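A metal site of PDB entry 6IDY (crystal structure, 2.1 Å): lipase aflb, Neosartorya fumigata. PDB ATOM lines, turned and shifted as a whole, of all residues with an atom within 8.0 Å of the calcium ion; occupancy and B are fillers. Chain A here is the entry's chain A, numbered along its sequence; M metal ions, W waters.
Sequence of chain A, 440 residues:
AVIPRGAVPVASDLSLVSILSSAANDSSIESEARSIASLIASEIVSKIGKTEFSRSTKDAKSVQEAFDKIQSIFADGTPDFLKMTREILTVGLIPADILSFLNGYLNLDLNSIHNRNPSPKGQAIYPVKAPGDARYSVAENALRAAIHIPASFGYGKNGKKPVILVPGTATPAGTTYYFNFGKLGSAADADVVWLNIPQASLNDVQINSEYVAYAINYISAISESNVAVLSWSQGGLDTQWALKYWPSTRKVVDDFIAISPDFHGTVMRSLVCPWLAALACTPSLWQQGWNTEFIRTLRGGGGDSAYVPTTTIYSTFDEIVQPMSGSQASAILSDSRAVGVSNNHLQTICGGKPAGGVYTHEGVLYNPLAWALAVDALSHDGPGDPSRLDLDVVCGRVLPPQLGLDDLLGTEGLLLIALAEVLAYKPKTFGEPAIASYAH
A ring nitrogen (ND1) of His 380 lies within hydrogen-bond range of the backbone carbonyl oxygen (O) of Asp 376, 2.8 Å away.
The side-chain hydroxyl (OG) of Ser 379 is in hydrogen-bond range of a ring nitrogen (ND1) of His 380, at 3.1 Å.
Residues that only touch the calcium ion: Asp 381.
Within 4 Å of the calcium ion: Asp 255, Ala 377, His 380, Asp 381 and Gly 382.
Along chain A the residues within 4 Å of the calcium ion span positions 255 to 382.
The nearest printed residue that does not touch the calcium ion is Asp 254 (4.3 Å).
The calcium ion is bound by the backbone carbonyl oxygen (O) of Ala 377 (2.2 Å), the backbone carbonyl oxygen (O) of His 380 (2.3 Å), water W1 (2.4 Å), the backbone carbonyl oxygen (O) of Gly 382 (2.4 Å), water W2 (2.4 Å), the side-chain carboxylate (OD1) of Asp 255 (2.4 Å) and the side-chain carboxylate (OD2) of Asp 255 (2.5 Å).
The calcium ion has seven donor atoms within binding distance.
Water W2 lies within hydrogen-bond range of O of Asp 254 and N of Gly 382.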
ATOM      1  N   LYS A 161      21.467  14.032  -5.958  1.00  0.00           N
ATOM      2  CA  LYS A 161      22.811  13.958  -5.404  1.00  0.00           C
ATOM      3  C   LYS A 161      22.775  13.357  -3.995  1.00  0.00           C
ATOM      4  O   LYS A 161      22.053  13.861  -3.150  1.00  0.00           O
ATOM      5  CB  LYS A 161      23.440  15.376  -5.374  1.00  0.00           C
ATOM      6  CG  LYS A 161      24.912  15.443  -4.950  1.00  0.00           C
ATOM      7  CD  LYS A 161      25.829  14.956  -6.056  1.00  0.00           C
ATOM      8  CE  LYS A 161      27.115  15.742  -6.086  1.00  0.00           C
ATOM      9  NZ  LYS A 161      27.015  16.918  -6.977  1.00  0.00           N
ATOM     10  N   ALA A 228      27.672  15.068  -1.556  1.00  0.00           N
ATOM     11  CA  ALA A 228      27.733  16.271  -0.766  1.00  0.00           C
ATOM     12  C   ALA A 228      27.667  15.819   0.681  1.00  0.00           C
ATOM     13  O   ALA A 228      27.147  14.742   0.988  1.00  0.00           O
ATOM     14  CB  ALA A 228      26.570  17.183  -1.097  1.00  0.00           C
ATOM     15  N   ASP A 254      31.667  17.105  -3.705  1.00  0.00           N
ATOM     16  CA  ASP A 254      31.447  18.340  -4.454  1.00  0.00           C
ATOM     17  C   ASP A 254      31.095  19.526  -3.560  1.00  0.00           C
ATOM     18  O   ASP A 254      31.368  20.663  -3.926  1.00  0.00           O
ATOM     19  CB  ASP A 254      30.368  18.158  -5.543  1.00  0.00           C
ATOM     20  CG  ASP A 254      30.755  17.199  -6.647  1.00  0.00           C
ATOM     21  OD1 ASP A 254      31.969  16.978  -6.861  1.00  0.00           O
ATOM     22  OD2 ASP A 254      29.842  16.674  -7.325  1.00  0.00           O
ATOM     23  N   ASP A 255      30.458  19.270  -2.413  1.00  0.00           N
ATOM     24  CA  ASP A 255      30.054  20.311  -1.480  1.00  0.00           C
ATOM     25  C   ASP A 255      30.125  19.830  -0.062  1.00  0.00           C
ATOM     26  O   ASP A 255      29.679  18.720   0.247  1.00  0.00           O
ATOM     27  CB  ASP A 255      28.620  20.796  -1.772  1.00  0.00           C
ATOM     28  CG  ASP A 255      28.496  21.705  -2.989  1.00  0.00           C
ATOM     29  OD1 ASP A 255      28.910  22.875  -2.905  1.00  0.00           O
ATOM     30  OD2 ASP A 255      27.951  21.237  -4.016  1.00  0.00           O
ATOM     31  N   PHE A 256      30.656  20.680   0.808  1.00  0.00           N
ATOM     32  CA  PHE A 256      30.711  20.444   2.242  1.00  0.00           C
ATOM     33  C   PHE A 256      29.964  21.623   2.865  1.00  0.00           C
ATOM     34  O   PHE A 256      30.452  22.745   2.835  1.00  0.00           O
ATOM     35  CB  PHE A 256      32.182  20.306   2.731  1.00  0.00           C
ATOM     36  CG  PHE A 256      32.490  20.270   4.227  1.00  0.00           C
ATOM     37  CD1 PHE A 256      31.489  19.985   5.156  1.00  0.00           C
ATOM     38  CD2 PHE A 256      33.784  20.500   4.693  1.00  0.00           C
ATOM     39  CE1 PHE A 256      31.779  19.970   6.530  1.00  0.00           C
ATOM     40  CE2 PHE A 256      34.067  20.473   6.065  1.00  0.00           C
ATOM     41  CZ  PHE A 256      33.059  20.206   6.971  1.00  0.00           C
ATOM     42  N   ILE A 257      28.722  21.382   3.324  1.00  0.00           N
ATOM     43  CA  ILE A 257      27.892  22.398   3.965  1.00  0.00           C
ATOM     44  C   ILE A 257      28.030  22.206   5.471  1.00  0.00           C
ATOM     45  O   ILE A 257      27.649  21.172   6.006  1.00  0.00           O
ATOM     46  CB  ILE A 257      26.408  22.366   3.454  1.00  0.00           C
ATOM     47  CG1 ILE A 257      26.360  22.548   1.915  1.00  0.00           C
ATOM     48  CG2 ILE A 257      25.546  23.428   4.181  1.00  0.00           C
ATOM     49  CD1 ILE A 257      25.224  21.780   1.214  1.00  0.00           C
ATOM     50  N   PRO A 309      34.728  22.507  -2.157  1.00  0.00           N
ATOM     51  CA  PRO A 309      33.876  23.705  -1.970  1.00  0.00           C
ATOM     52  C   PRO A 309      33.122  23.643  -0.632  1.00  0.00           C
ATOM     53  O   PRO A 309      32.344  22.714  -0.416  1.00  0.00           O
ATOM     54  CB  PRO A 309      32.924  23.643  -3.169  1.00  0.00           C
ATOM     55  CG  PRO A 309      33.731  22.945  -4.237  1.00  0.00           C
ATOM     56  CD  PRO A 309      34.468  21.872  -3.466  1.00  0.00           C
ATOM     57  N   THR A 310      33.440  24.575   0.286  1.00  0.00           N
ATOM     58  CA  THR A 310      32.833  24.572   1.624  1.00  0.00           C
ATOM     59  C   THR A 310      31.980  25.813   1.876  1.00  0.00           C
ATOM     60  O   THR A 310      32.415  26.943   1.616  1.00  0.00           O
ATOM     61  CB  THR A 310      33.897  24.347   2.721  1.00  0.00           C
ATOM     62  OG1 THR A 310      34.650  23.171   2.396  1.00  0.00           O
ATOM     63  CG2 THR A 310      33.290  24.191   4.116  1.00  0.00           C
ATOM     64  N   THR A 311      30.757  25.589   2.394  1.00  0.00           N
ATOM     65  CA  THR A 311      29.783  26.608   2.755  1.00  0.00           C
ATOM     66  C   THR A 311      29.599  26.532   4.284  1.00  0.00           C
ATOM     67  O   THR A 311      28.964  25.599   4.780  1.00  0.00           O
ATOM     68  CB  THR A 311      28.467  26.350   1.995  1.00  0.00           C
ATOM     69  OG1 THR A 311      28.737  26.216   0.602  1.00  0.00           O
ATOM     70  CG2 THR A 311      27.418  27.439   2.238  1.00  0.00           C
ATOM     71  N   LEU A 373      21.215  28.834   1.468  1.00  0.00           N
ATOM     72  CA  LEU A 373      22.627  28.667   1.112  1.00  0.00           C
ATOM     73  C   LEU A 373      22.943  27.216   0.776  1.00  0.00           C
ATOM     74  O   LEU A 373      23.712  26.968  -0.148  1.00  0.00           O
ATOM     75  CB  LEU A 373      23.545  29.181   2.224  1.00  0.00           C
ATOM     76  CG  LEU A 373      23.659  30.700   2.339  1.00  0.00           C
ATOM     77  CD1 LEU A 373      24.142  31.083   3.701  1.00  0.00           C
ATOM     78  CD2 LEU A 373      24.531  31.305   1.222  1.00  0.00           C
ATOM     79  N   ALA A 374      22.340  26.259   1.514  1.00  0.00           N
ATOM     80  CA  ALA A 374      22.534  24.823   1.264  1.00  0.00           C
ATOM     81  C   ALA A 374      22.011  24.469  -0.131  1.00  0.00           C
ATOM     82  O   ALA A 374      22.703  23.786  -0.878  1.00  0.00           O
ATOM     83  CB  ALA A 374      21.805  24.002   2.324  1.00  0.00           C
ATOM     84  N   VAL A 375      20.817  24.969  -0.500  1.00  0.00           N
ATOM     85  CA  VAL A 375      20.141  24.767  -1.792  1.00  0.00           C
ATOM     86  C   VAL A 375      20.984  25.397  -2.907  1.00  0.00           C
ATOM     87  O   VAL A 375      21.259  24.743  -3.920  1.00  0.00           O
ATOM     88  CB  VAL A 375      18.674  25.288  -1.767  1.00  0.00           C
ATOM     89  CG1 VAL A 375      18.052  25.301  -3.158  1.00  0.00           C
ATOM     90  CG2 VAL A 375      17.830  24.455  -0.809  1.00  0.00           C
ATOM     91  N   ASP A 376      21.434  26.642  -2.702  1.00  0.00           N
ATOM     92  CA  ASP A 376      22.280  27.351  -3.665  1.00  0.00           C
ATOM     93  C   ASP A 376      23.638  26.630  -3.883  1.00  0.00           C
ATOM     94  O   ASP A 376      24.081  26.540  -5.026  1.00  0.00           O
ATOM     95  CB  ASP A 376      22.479  28.811  -3.250  1.00  0.00           C
ATOM     96  CG  ASP A 376      23.374  29.585  -4.183  1.00  0.00           C
ATOM     97  OD1 ASP A 376      22.863  30.075  -5.221  1.00  0.00           O
ATOM     98  OD2 ASP A 376      24.580  29.661  -3.911  1.00  0.00           O
ATOM     99  N   ALA A 377      24.254  26.097  -2.801  1.00  0.00           N
ATOM    100  CA  ALA A 377      25.522  25.359  -2.871  1.00  0.00           C
ATOM    101  C   ALA A 377      25.389  24.094  -3.720  1.00  0.00           C
ATOM    102  O   ALA A 377      26.259  23.804  -4.528  1.00  0.00           O
ATOM    103  CB  ALA A 377      25.976  24.974  -1.468  1.00  0.00           C
ATOM    104  N   LEU A 378      24.283  23.351  -3.522  1.00  0.00           N
ATOM    105  CA  LEU A 378      24.010  22.097  -4.228  1.00  0.00           C
ATOM    106  C   LEU A 378      23.642  22.295  -5.705  1.00  0.00           C
ATOM    107  O   LEU A 378      23.832  21.361  -6.484  1.00  0.00           O
ATOM    108  CB  LEU A 378      22.918  21.307  -3.499  1.00  0.00           C
ATOM    109  CG  LEU A 378      23.304  20.780  -2.104  1.00  0.00           C
ATOM    110  CD1 LEU A 378      22.090  20.332  -1.349  1.00  0.00           C
ATOM    111  CD2 LEU A 378      24.329  19.671  -2.198  1.00  0.00           C
ATOM    112  N   SER A 379      23.145  23.475  -6.086  1.00  0.00           N
ATOM    113  CA  SER A 379      22.726  23.768  -7.460  1.00  0.00           C
ATOM    114  C   SER A 379      23.782  24.482  -8.309  1.00  0.00           C
ATOM    115  O   SER A 379      23.580  24.640  -9.511  1.00  0.00           O
ATOM    116  CB  SER A 379      21.401  24.529  -7.461  1.00  0.00           C
ATOM    117  OG  SER A 379      21.516  25.763  -6.757  1.00  0.00           O
ATOM    118  N   HIS A 380      24.903  24.891  -7.703  1.00  0.00           N
ATOM    119  CA  HIS A 380      25.960  25.601  -8.426  1.00  0.00           C
ATOM    120  C   HIS A 380      27.331  25.007  -8.149  1.00  0.00           C
ATOM    121  O   HIS A 380      27.565  24.502  -7.057  1.00  0.00           O
ATOM    122  CB  HIS A 380      25.992  27.081  -8.014  1.00  0.00           C
ATOM    123  CG  HIS A 380      24.737  27.836  -8.340  1.00  0.00           C
ATOM    124  ND1 HIS A 380      23.659  27.849  -7.477  1.00  0.00           N
ATOM    125  CD2 HIS A 380      24.427  28.580  -9.426  1.00  0.00           C
ATOM    126  CE1 HIS A 380      22.737  28.595  -8.062  1.00  0.00           C
ATOM    127  NE2 HIS A 380      23.156  29.054  -9.242  1.00  0.00           N
ATOM    128  N   ASP A 381      28.268  25.140  -9.127  1.00  0.00           N
ATOM    129  CA  ASP A 381      29.668  24.746  -8.927  1.00  0.00           C
ATOM    130  C   ASP A 381      30.201  25.687  -7.851  1.00  0.00           C
ATOM    131  O   ASP A 381      29.808  26.850  -7.796  1.00  0.00           O
ATOM    132  CB  ASP A 381      30.491  24.909 -10.226  1.00  0.00           C
ATOM    133  CG  ASP A 381      30.126  23.975 -11.382  1.00  0.00           C
ATOM    134  OD1 ASP A 381      29.628  22.861 -11.112  1.00  0.00           O
ATOM    135  OD2 ASP A 381      30.371  24.360 -12.539  1.00  0.00           O
ATOM    136  N   GLY A 382      31.023  25.156  -6.954  1.00  0.00           N
ATOM    137  CA  GLY A 382      31.546  25.932  -5.847  1.00  0.00           C
ATOM    138  C   GLY A 382      30.575  26.005  -4.681  1.00  0.00           C
ATOM    139  O   GLY A 382      29.552  25.315  -4.665  1.00  0.00           O
ATOM    140  N   PRO A 383      30.880  26.856  -3.666  1.00  0.00           N
ATOM    141  CA  PRO A 383      30.010  26.934  -2.477  1.00  0.00           C
ATOM    142  C   PRO A 383      28.740  27.774  -2.667  1.00  0.00           C
ATOM    143  O   PRO A 383      28.519  28.356  -3.730  1.00  0.00           O
ATOM    144  CB  PRO A 383      30.941  27.562  -1.429  1.00  0.00           C
ATOM    145  CG  PRO A 383      31.815  28.469  -2.247  1.00  0.00           C
ATOM    146  CD  PRO A 383      32.050  27.753  -3.540  1.00  0.00           C
ATOM    147  N   GLY A 384      27.939  27.834  -1.603  1.00  0.00           N
ATOM    148  CA  GLY A 384      26.739  28.670  -1.549  1.00  0.00           C
ATOM    149  C   GLY A 384      27.147  30.122  -1.602  1.00  0.00           C
ATOM    150  O   GLY A 384      28.179  30.486  -1.050  1.00  0.00           O
ATOM    151  N   ARG A 388      23.629  35.388  -4.882  1.00  0.00           N
ATOM    152  CA  ARG A 388      22.729  34.721  -5.836  1.00  0.00           C
ATOM    153  C   ARG A 388      21.338  34.541  -5.245  1.00  0.00           C
ATOM    154  O   ARG A 388      20.429  34.067  -5.941  1.00  0.00           O
ATOM    155  CB  ARG A 388      23.281  33.346  -6.249  1.00  0.00           C
ATOM    156  CG  ARG A 388      24.443  33.390  -7.239  1.00  0.00           C
ATOM    157  CD  ARG A 388      24.675  32.019  -7.864  1.00  0.00           C
ATOM    158  NE  ARG A 388      25.077  31.015  -6.875  1.00  0.00           N
ATOM    159  CZ  ARG A 388      26.298  30.501  -6.761  1.00  0.00           C
ATOM    160  NH1 ARG A 388      27.260  30.883  -7.593  1.00  0.00           N
ATOM    161  NH2 ARG A 388      26.565  29.595  -5.834  1.00  0.00           N
HETATM  162 CA    CA M   1      28.317  23.342  -5.228  1.00  0.00          CA
HETATM  163  O   HOH W   1      27.479  21.789  -6.781  1.00  0.00           O
HETATM  164  O   HOH W   2      30.409  22.325  -5.825  1.00  0.00           O
